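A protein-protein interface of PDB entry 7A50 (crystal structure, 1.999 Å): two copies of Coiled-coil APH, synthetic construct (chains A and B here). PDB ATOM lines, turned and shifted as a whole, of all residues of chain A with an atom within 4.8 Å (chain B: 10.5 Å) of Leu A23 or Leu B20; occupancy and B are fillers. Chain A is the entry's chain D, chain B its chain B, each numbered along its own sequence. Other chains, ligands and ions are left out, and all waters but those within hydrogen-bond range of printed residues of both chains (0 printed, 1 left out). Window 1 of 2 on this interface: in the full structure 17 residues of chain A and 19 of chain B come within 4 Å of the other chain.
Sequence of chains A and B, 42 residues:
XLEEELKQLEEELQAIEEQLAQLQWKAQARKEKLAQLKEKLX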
ATOM      1  N   GLN A  19     -26.817   6.648  10.366  1.00  0.00           N
ATOM      2  CA  GLN A  19     -25.952   6.047   9.349  1.00  0.00           C
ATOM      3  C   GLN A  19     -24.556   5.777   9.900  1.00  0.00           C
ATOM      4  O   GLN A  19     -23.991   4.691   9.699  1.00  0.00           O
ATOM      5  CB  GLN A  19     -25.858   6.965   8.139  1.00  0.00           C
ATOM      6  CG  GLN A  19     -27.155   7.181   7.389  1.00  0.00           C
ATOM      7  CD  GLN A  19     -27.012   8.344   6.410  1.00  0.00           C
ATOM      8  OE1 GLN A  19     -26.386   8.202   5.351  1.00  0.00           O
ATOM      9  NE2 GLN A  19     -27.566   9.509   6.771  1.00  0.00           N
ATOM     10  N   LEU A  20     -23.970   6.767  10.579  1.00  0.00           N
ATOM     11  CA  LEU A  20     -22.636   6.583  11.143  1.00  0.00           C
ATOM     12  C   LEU A  20     -22.602   5.426  12.133  1.00  0.00           C
ATOM     13  O   LEU A  20     -21.635   4.660  12.158  1.00  0.00           O
ATOM     14  CB  LEU A  20     -22.163   7.863  11.823  1.00  0.00           C
ATOM     15  CG  LEU A  20     -21.887   9.085  10.943  1.00  0.00           C
ATOM     16  CD1 LEU A  20     -21.635  10.320  11.830  1.00  0.00           C
ATOM     17  CD2 LEU A  20     -20.722   8.826   9.980  1.00  0.00           C
ATOM     18  N   ALA A  21     -23.628   5.301  12.986  1.00  0.00           N
ATOM     19  CA  ALA A  21     -23.645   4.210  13.958  1.00  0.00           C
ATOM     20  C   ALA A  21     -23.572   2.850  13.271  1.00  0.00           C
ATOM     21  O   ALA A  21     -22.786   1.988  13.671  1.00  0.00           O
ATOM     22  CB  ALA A  21     -24.894   4.281  14.831  1.00  0.00           C
ATOM     23  N   GLN A  22     -24.396   2.630  12.248  1.00  0.00           N
ATOM     24  CA  GLN A  22     -24.381   1.327  11.595  1.00  0.00           C
ATOM     25  C   GLN A  22     -23.097   1.120  10.785  1.00  0.00           C
ATOM     26  O   GLN A  22     -22.527   0.017  10.782  1.00  0.00           O
ATOM     27  CB  GLN A  22     -25.604   1.154  10.703  1.00  0.00           C
ATOM     28  CG  GLN A  22     -25.606  -0.231  10.053  1.00  0.00           C
ATOM     29  CD  GLN A  22     -26.586  -0.370   8.910  1.00  0.00           C
ATOM     30  OE1 GLN A  22     -26.306   0.066   7.785  1.00  0.00           O
ATOM     31  NE2 GLN A  22     -27.715  -1.017   9.172  1.00  0.00           N
ATOM     32  N   LEU A  23     -22.648   2.153  10.061  1.00  0.00           N
ATOM     33  CA  LEU A  23     -21.456   1.985   9.228  1.00  0.00           C
ATOM     34  C   LEU A  23     -20.212   1.735  10.075  1.00  0.00           C
ATOM     35  O   LEU A  23     -19.349   0.931   9.692  1.00  0.00           O
ATOM     36  CB  LEU A  23     -21.267   3.200   8.326  1.00  0.00           C
ATOM     37  CG  LEU A  23     -22.340   3.304   7.244  1.00  0.00           C
ATOM     38  CD1 LEU A  23     -22.283   4.711   6.594  1.00  0.00           C
ATOM     39  CD2 LEU A  23     -22.116   2.237   6.221  1.00  0.00           C
ATOM     40  N   GLN A  24     -20.098   2.406  11.229  1.00  0.00           N
ATOM     41  CA  GLN A  24     -18.950   2.154  12.105  1.00  0.00           C
ATOM     42  C   GLN A  24     -18.983   0.730  12.662  1.00  0.00           C
ATOM     43  O   GLN A  24     -17.931   0.091  12.818  1.00  0.00           O
ATOM     44  CB  GLN A  24     -18.941   3.176  13.224  1.00  0.00           C
ATOM     45  CG  GLN A  24     -18.669   4.588  12.662  1.00  0.00           C
ATOM     46  CD  GLN A  24     -18.821   5.691  13.704  1.00  0.00           C
ATOM     47  OE1 GLN A  24     -19.241   5.439  14.837  1.00  0.00           O
ATOM     48  NE2 GLN A  24     -18.535   6.931  13.304  1.00  0.00           N
ATOM     49  N   TRP A  25     -20.180   0.217  12.970  1.00  0.00           N
ATOM     50  CA  TRP A  25     -20.280  -1.175  13.392  1.00  0.00           C
ATOM     51  C   TRP A  25     -19.905  -2.111  12.245  1.00  0.00           C
ATOM     52  O   TRP A  25     -19.141  -3.067  12.442  1.00  0.00           O
ATOM     53  CB  TRP A  25     -21.685  -1.468  13.921  1.00  0.00           C
ATOM     54  CG  TRP A  25     -21.742  -2.894  14.344  1.00  0.00           C
ATOM     55  CD1 TRP A  25     -21.403  -3.397  15.569  1.00  0.00           C
ATOM     56  CD2 TRP A  25     -22.130  -4.015  13.538  1.00  0.00           C
ATOM     57  NE1 TRP A  25     -21.548  -4.771  15.570  1.00  0.00           N
ATOM     58  CE2 TRP A  25     -21.999  -5.171  14.339  1.00  0.00           C
ATOM     59  CE3 TRP A  25     -22.580  -4.151  12.218  1.00  0.00           C
ATOM     60  CZ2 TRP A  25     -22.304  -6.459  13.861  1.00  0.00           C
ATOM     61  CZ3 TRP A  25     -22.879  -5.435  11.746  1.00  0.00           C
ATOM     62  CH2 TRP A  25     -22.729  -6.565  12.563  1.00  0.00           C
ATOM     63  N   LYS A  26     -20.391  -1.818  11.030  1.00  0.00           N
ATOM     64  CA  LYS A  26     -20.045  -2.621   9.854  1.00  0.00           C
ATOM     65  C   LYS A  26     -18.540  -2.624   9.592  1.00  0.00           C
ATOM     66  O   LYS A  26     -17.970  -3.661   9.213  1.00  0.00           O
ATOM     67  CB  LYS A  26     -20.820  -2.124   8.626  1.00  0.00           C
ATOM     68  CG  LYS A  26     -22.286  -2.642   8.571  1.00  0.00           C
ATOM     69  CD  LYS A  26     -23.067  -2.141   7.328  1.00  0.00           C
ATOM     70  CE  LYS A  26     -24.465  -2.741   7.306  1.00  0.00           C
ATOM     71  NZ  LYS A  26     -25.312  -2.252   6.173  1.00  0.00           N
ATOM     72  N   ALA A  27     -17.881  -1.478   9.772  1.00  0.00           N
ATOM     73  CA  ALA A  27     -16.433  -1.394   9.578  1.00  0.00           C
ATOM     74  C   ALA A  27     -15.688  -2.158  10.666  1.00  0.00           C
ATOM     75  O   ALA A  27     -14.749  -2.915  10.380  1.00  0.00           O
ATOM     76  CB  ALA A  27     -15.970   0.069   9.537  1.00  0.00           C
ATOM     77  N   GLU B  12     -14.822  -3.717   0.740  1.00  0.00           N
ATOM     78  CA  GLU B  12     -15.928  -3.244   1.560  1.00  0.00           C
ATOM     79  C   GLU B  12     -15.453  -2.197   2.551  1.00  0.00           C
ATOM     80  O   GLU B  12     -16.090  -1.154   2.714  1.00  0.00           O
ATOM     81  CB  GLU B  12     -16.582  -4.437   2.270  1.00  0.00           C
ATOM     82  CG  GLU B  12     -17.410  -5.256   1.314  1.00  0.00           C
ATOM     83  CD  GLU B  12     -18.039  -6.456   1.971  1.00  0.00           C
ATOM     84  OE1 GLU B  12     -17.528  -6.870   3.039  1.00  0.00           O
ATOM     85  OE2 GLU B  12     -19.034  -6.972   1.417  1.00  0.00           O
ATOM     86  N   LEU B  13     -14.340  -2.469   3.233  1.00  0.00           N
ATOM     87  CA  LEU B  13     -13.799  -1.498   4.174  1.00  0.00           C
ATOM     88  C   LEU B  13     -13.466  -0.172   3.490  1.00  0.00           C
ATOM     89  O   LEU B  13     -13.711   0.907   4.052  1.00  0.00           O
ATOM     90  CB  LEU B  13     -12.582  -2.075   4.887  1.00  0.00           C
ATOM     91  CG  LEU B  13     -12.953  -2.978   6.060  1.00  0.00           C
ATOM     92  CD1 LEU B  13     -11.733  -3.812   6.474  1.00  0.00           C
ATOM     93  CD2 LEU B  13     -13.461  -2.097   7.219  1.00  0.00           C
ATOM     94  N   GLN B  14     -12.927  -0.220   2.269  1.00  0.00           N
ATOM     95  CA  GLN B  14     -12.657   1.030   1.570  1.00  0.00           C
ATOM     96  C   GLN B  14     -13.942   1.796   1.267  1.00  0.00           C
ATOM     97  O   GLN B  14     -13.982   3.028   1.409  1.00  0.00           O
ATOM     98  CB  GLN B  14     -11.900   0.767   0.275  1.00  0.00           C
ATOM     99  CG  GLN B  14     -11.496   2.024  -0.470  1.00  0.00           C
ATOM    100  CD  GLN B  14     -11.032   1.680  -1.890  1.00  0.00           C
ATOM    101  OE1 GLN B  14     -11.696   2.019  -2.873  1.00  0.00           O
ATOM    102  NE2 GLN B  14      -9.901   0.979  -1.997  1.00  0.00           N
ATOM    103  N   ALA B  15     -14.991   1.092   0.816  1.00  0.00           N
ATOM    104  CA  ALA B  15     -16.280   1.746   0.569  1.00  0.00           C
ATOM    105  C   ALA B  15     -16.865   2.329   1.857  1.00  0.00           C
ATOM    106  O   ALA B  15     -17.427   3.433   1.856  1.00  0.00           O
ATOM    107  CB  ALA B  15     -17.266   0.756  -0.063  1.00  0.00           C
ATOM    108  N   ILE B  16     -16.725   1.613   2.969  1.00  0.00           N
ATOM    109  CA  ILE B  16     -17.232   2.137   4.228  1.00  0.00           C
ATOM    110  C   ILE B  16     -16.448   3.375   4.646  1.00  0.00           C
ATOM    111  O   ILE B  16     -17.032   4.365   5.114  1.00  0.00           O
ATOM    112  CB  ILE B  16     -17.216   1.043   5.313  1.00  0.00           C
ATOM    113  CG1 ILE B  16     -18.233  -0.053   4.965  1.00  0.00           C
ATOM    114  CG2 ILE B  16     -17.546   1.639   6.668  1.00  0.00           C
ATOM    115  CD1 ILE B  16     -18.070  -1.338   5.782  1.00  0.00           C
ATOM    116  N   GLU B  17     -15.126   3.367   4.443  1.00  0.00           N
ATOM    117  CA  GLU B  17     -14.324   4.534   4.798  1.00  0.00           C
ATOM    118  C   GLU B  17     -14.683   5.766   3.957  1.00  0.00           C
ATOM    119  O   GLU B  17     -14.648   6.896   4.474  1.00  0.00           O
ATOM    120  CB  GLU B  17     -12.831   4.222   4.681  1.00  0.00           C
ATOM    121  CG  GLU B  17     -12.356   3.215   5.727  1.00  0.00           C
ATOM    122  CD  GLU B  17     -12.733   3.588   7.167  1.00  0.00           C
ATOM    123  OE1 GLU B  17     -12.868   4.791   7.490  1.00  0.00           O
ATOM    124  OE2 GLU B  17     -12.912   2.657   7.985  1.00  0.00           O
ATOM    125  N   GLU B  18     -14.983   5.583   2.657  1.00  0.00           N
ATOM    126  CA  GLU B  18     -15.428   6.709   1.824  1.00  0.00           C
ATOM    127  C   GLU B  18     -16.792   7.252   2.278  1.00  0.00           C
ATOM    128  O   GLU B  18     -17.032   8.470   2.220  1.00  0.00           O
ATOM    129  CB  GLU B  18     -15.510   6.300   0.356  1.00  0.00           C
ATOM    130  CG  GLU B  18     -14.235   5.653  -0.173  1.00  0.00           C
ATOM    131  CD  GLU B  18     -14.346   5.179  -1.623  1.00  0.00           C
ATOM    132  OE1 GLU B  18     -15.444   5.306  -2.218  1.00  0.00           O
ATOM    133  OE2 GLU B  18     -13.335   4.654  -2.154  1.00  0.00           O
ATOM    134  N   GLN B  19     -17.714   6.360   2.671  1.00  0.00           N
ATOM    135  CA  GLN B  19     -19.002   6.801   3.202  1.00  0.00           C
ATOM    136  C   GLN B  19     -18.823   7.579   4.497  1.00  0.00           C
ATOM    137  O   GLN B  19     -19.365   8.682   4.651  1.00  0.00           O
ATOM    138  CB  GLN B  19     -19.928   5.604   3.447  1.00  0.00           C
ATOM    139  CG  GLN B  19     -20.369   4.865   2.217  1.00  0.00           C
ATOM    140  CD  GLN B  19     -21.065   3.556   2.583  1.00  0.00           C
ATOM    141  OE1 GLN B  19     -22.213   3.574   3.022  1.00  0.00           O
ATOM    142  NE2 GLN B  19     -20.361   2.412   2.424  1.00  0.00           N
ATOM    143  N   LEU B  20     -18.036   7.027   5.431  1.00  0.00           N
ATOM    144  CA  LEU B  20     -17.801   7.685   6.713  1.00  0.00           C
ATOM    145  C   LEU B  20     -17.177   9.063   6.538  1.00  0.00           C
ATOM    146  O   LEU B  20     -17.565  10.021   7.225  1.00  0.00           O
ATOM    147  CB  LEU B  20     -16.910   6.803   7.589  1.00  0.00           C
ATOM    148  CG  LEU B  20     -17.642   5.516   8.036  1.00  0.00           C
ATOM    149  CD1 LEU B  20     -16.676   4.569   8.727  1.00  0.00           C
ATOM    150  CD2 LEU B  20     -18.782   5.862   8.971  1.00  0.00           C
ATOM    151  N   ALA B  21     -16.198   9.180   5.632  1.00  0.00           N
ATOM    152  CA  ALA B  21     -15.566  10.468   5.388  1.00  0.00           C
ATOM    153  C   ALA B  21     -16.598  11.500   4.958  1.00  0.00           C
ATOM    154  O   ALA B  21     -16.594  12.629   5.453  1.00  0.00           O
ATOM    155  CB  ALA B  21     -14.456  10.343   4.335  1.00  0.00           C
ATOM    156  N   GLN B  22     -17.482  11.132   4.027  1.00  0.00           N
ATOM    157  CA  GLN B  22     -18.470  12.087   3.538  1.00  0.00           C
ATOM    158  C   GLN B  22     -19.521  12.385   4.597  1.00  0.00           C
ATOM    159  O   GLN B  22     -19.828  13.555   4.866  1.00  0.00           O
ATOM    160  CB  GLN B  22     -19.147  11.583   2.261  1.00  0.00           C
ATOM    161  CG  GLN B  22     -20.090  12.651   1.711  1.00  0.00           C
ATOM    162  CD  GLN B  22     -21.033  12.179   0.620  1.00  0.00           C
ATOM    163  OE1 GLN B  22     -22.112  11.642   0.892  1.00  0.00           O
ATOM    164  NE2 GLN B  22     -20.615  12.365  -0.637  1.00  0.00           N
ATOM    165  N   LEU B  23     -20.046  11.338   5.248  1.00  0.00           N
ATOM    166  CA  LEU B  23     -21.119  11.533   6.227  1.00  0.00           C
ATOM    167  C   LEU B  23     -20.650  12.359   7.410  1.00  0.00           C
ATOM    168  O   LEU B  23     -21.392  13.214   7.900  1.00  0.00           O
ATOM    169  CB  LEU B  23     -21.675  10.184   6.700  1.00  0.00           C
ATOM    170  CG  LEU B  23     -22.496   9.510   5.584  1.00  0.00           C
ATOM    171  CD1 LEU B  23     -22.786   8.063   5.899  1.00  0.00           C
ATOM    172  CD2 LEU B  23     -23.806  10.257   5.400  1.00  0.00           C
ATOM    173  N   GLN B  24     -19.401  12.161   7.847  1.00  0.00           N
ATOM    174  CA  GLN B  24     -18.875  12.963   8.948  1.00  0.00           C
ATOM    175  C   GLN B  24     -18.693  14.425   8.563  1.00  0.00           C
ATOM    176  O   GLN B  24     -18.922  15.312   9.391  1.00  0.00           O
ATOM    177  CB  GLN B  24     -17.565  12.376   9.456  1.00  0.00           C
ATOM    178  CG  GLN B  24     -17.921  11.054  10.098  1.00  0.00           C
ATOM    179  CD  GLN B  24     -16.877  10.501  10.999  1.00  0.00           C
ATOM    180  OE1 GLN B  24     -15.820  10.038  10.556  1.00  0.00           O
ATOM    181  NE2 GLN B  24     -17.175  10.520  12.303  1.00  0.00           N
ATOM    182  N   TRP B  25     -18.261  14.693   7.327  1.00  0.00           N
ATOM    183  CA  TRP B  25     -18.164  16.079   6.869  1.00  0.00           C
ATOM    184  C   TRP B  25     -19.548  16.710   6.793  1.00  0.00           C
ATOM    185  O   TRP B  25     -19.761  17.844   7.265  1.00  0.00           O
ATOM    186  CB  TRP B  25     -17.449  16.123   5.515  1.00  0.00           C
ATOM    187  CG  TRP B  25     -17.343  17.505   4.993  1.00  0.00           C
ATOM    188  CD1 TRP B  25     -16.323  18.383   5.200  1.00  0.00           C
ATOM    189  CD2 TRP B  25     -18.325  18.196   4.221  1.00  0.00           C
ATOM    190  NE1 TRP B  25     -16.610  19.586   4.595  1.00  0.00           N
ATOM    191  CE2 TRP B  25     -17.831  19.495   3.982  1.00  0.00           C
ATOM    192  CE3 TRP B  25     -19.565  17.838   3.689  1.00  0.00           C
ATOM    193  CZ2 TRP B  25     -18.531  20.433   3.228  1.00  0.00           C
ATOM    194  CZ3 TRP B  25     -20.273  18.790   2.950  1.00  0.00           C
ATOM    195  CH2 TRP B  25     -19.752  20.064   2.735  1.00  0.00           C
ATOM    196  N   LYS B  26     -20.521  15.954   6.268  1.00  0.00           N
ATOM    197  CA  LYS B  26     -21.899  16.438   6.207  1.00  0.00           C
ATOM    198  C   LYS B  26     -22.445  16.760   7.593  1.00  0.00           C
ATOM    199  O   LYS B  26     -23.130  17.787   7.781  1.00  0.00           O
ATOM    200  CB  LYS B  26     -22.776  15.402   5.510  1.00  0.00           C
ATOM    201  CG  LYS B  26     -22.597  15.407   3.966  1.00  0.00           C
ATOM    202  CD  LYS B  26     -23.556  14.439   3.278  1.00  0.00           C
ATOM    203  CE  LYS B  26     -23.455  14.549   1.769  1.00  0.00           C
ATOM    204  NZ  LYS B  26     -24.374  13.635   1.074  1.00  0.00           N
ATOM    205  N   ALA B  27     -22.137  15.909   8.580  1.00  0.00           N
ATOM    206  CA  ALA B  27     -22.587  16.155   9.950  1.00  0.00           C
ATOM    207  C   ALA B  27     -21.903  17.386  10.530  1.00  0.00           C
ATOM    208  O   ALA B  27     -22.561  18.239  11.121  1.00  0.00           O
ATOM    209  CB  ALA B  27     -22.323  14.937  10.846  1.00  0.00           C
ATOM    210  N   GLN B  28     -20.582  17.496  10.360  1.00  0.00           N
ATOM    211  CA  GLN B  28     -19.866  18.641  10.911  1.00  0.00           C
ATOM    212  C   GLN B  28     -20.381  19.955  10.329  1.00  0.00           C
ATOM    213  O   GLN B  28     -20.570  20.940  11.060  1.00  0.00           O
ATOM    214  CB  GLN B  28     -18.367  18.487  10.665  1.00  0.00           C
ATOM    215  CG  GLN B  28     -17.494  19.605  11.279  1.00  0.00           C
ATOM    216  CD  GLN B  28     -17.796  19.849  12.773  1.00  0.00           C
ATOM    217  OE1 GLN B  28     -18.290  18.957  13.484  1.00  0.00           O
ATOM    218  NE2 GLN B  28     -17.494  21.066  13.252  1.00  0.00           N
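Leu A23 touches four residues of chain B. Leu A20 touches just these residues of chain B: Leu B20 (3.7 Å), Leu B23 (3.7 Å) and Gln B24 (3.6 Å). No residue of chain B comes within 4 Å of Ala A21. No residue of chain B comes within 4 Å of Gln A22. Of chain B, only Leu B20 and Gln B24 come within 4 Å of Gln A24. No residue of chain B comes within 4 Å of Lys A26. Printed residues of chain A within 4 Å of Ile B16: Leu A23 (3.6 Å) and Ala A27 (3.6 Å). Printed residues of chain A within 4 Å of Leu B13: Ala A27. Of the printed residues of chain A, Gln B24 touches Leu A20 and Gln A24. Of the printed residues of chain A, Gln B19 touches Leu A23. Glu B18 touches none of the printed residues of chain A. The nearest residue of chain B that does not touch Leu A23 is Ala B15 (6.5 Å).
Among the printed residues, pairs that only touch across the chains: Gln A19 with Leu B23, Leu A20 with Leu B20, Leu A20 with Leu B23, Leu A20 with Gln B24, Leu A23 with Ile B16, Leu A23 with Gln B19, Leu A23 with Leu B20, Leu A23 with Leu B23, Gln A24 with Leu B20, Gln A24 with Gln B24, Ala A27 with Leu B13 and Ala A27 with Ile B16.
Gln A19 touches Leu B23, and with the chains exchanged Leu A23 touches Gln B19. Leu B20 touches its own counterpart, Leu A20. Leu A20 touches Leu B23, and with the chains exchanged Leu A23 touches Leu B20. Gln B24 touches its own counterpart, Gln A24. Of the 12 pairs that touch across the chains among the printed residues, 9 have their exchanged pair printed and touching as well.
Of the 17 printed residues of chain B, 6 touch a printed residue of chain A. Hydrophobic or aromatic side chains of chain A that line the printed part of chain B: Leu A20, Leu A23 and Ala A27. Among the printed residues, 12 pairs touch across the chains. Among the printed residues, no Asp or Glu carboxylate lies within 4 Å of a Lys or Arg side-chain nitrogen of the other chain.
O of Ala B15 lies within hydrogen-bond range of NE2 of Gln B19, at 3.2 Å.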
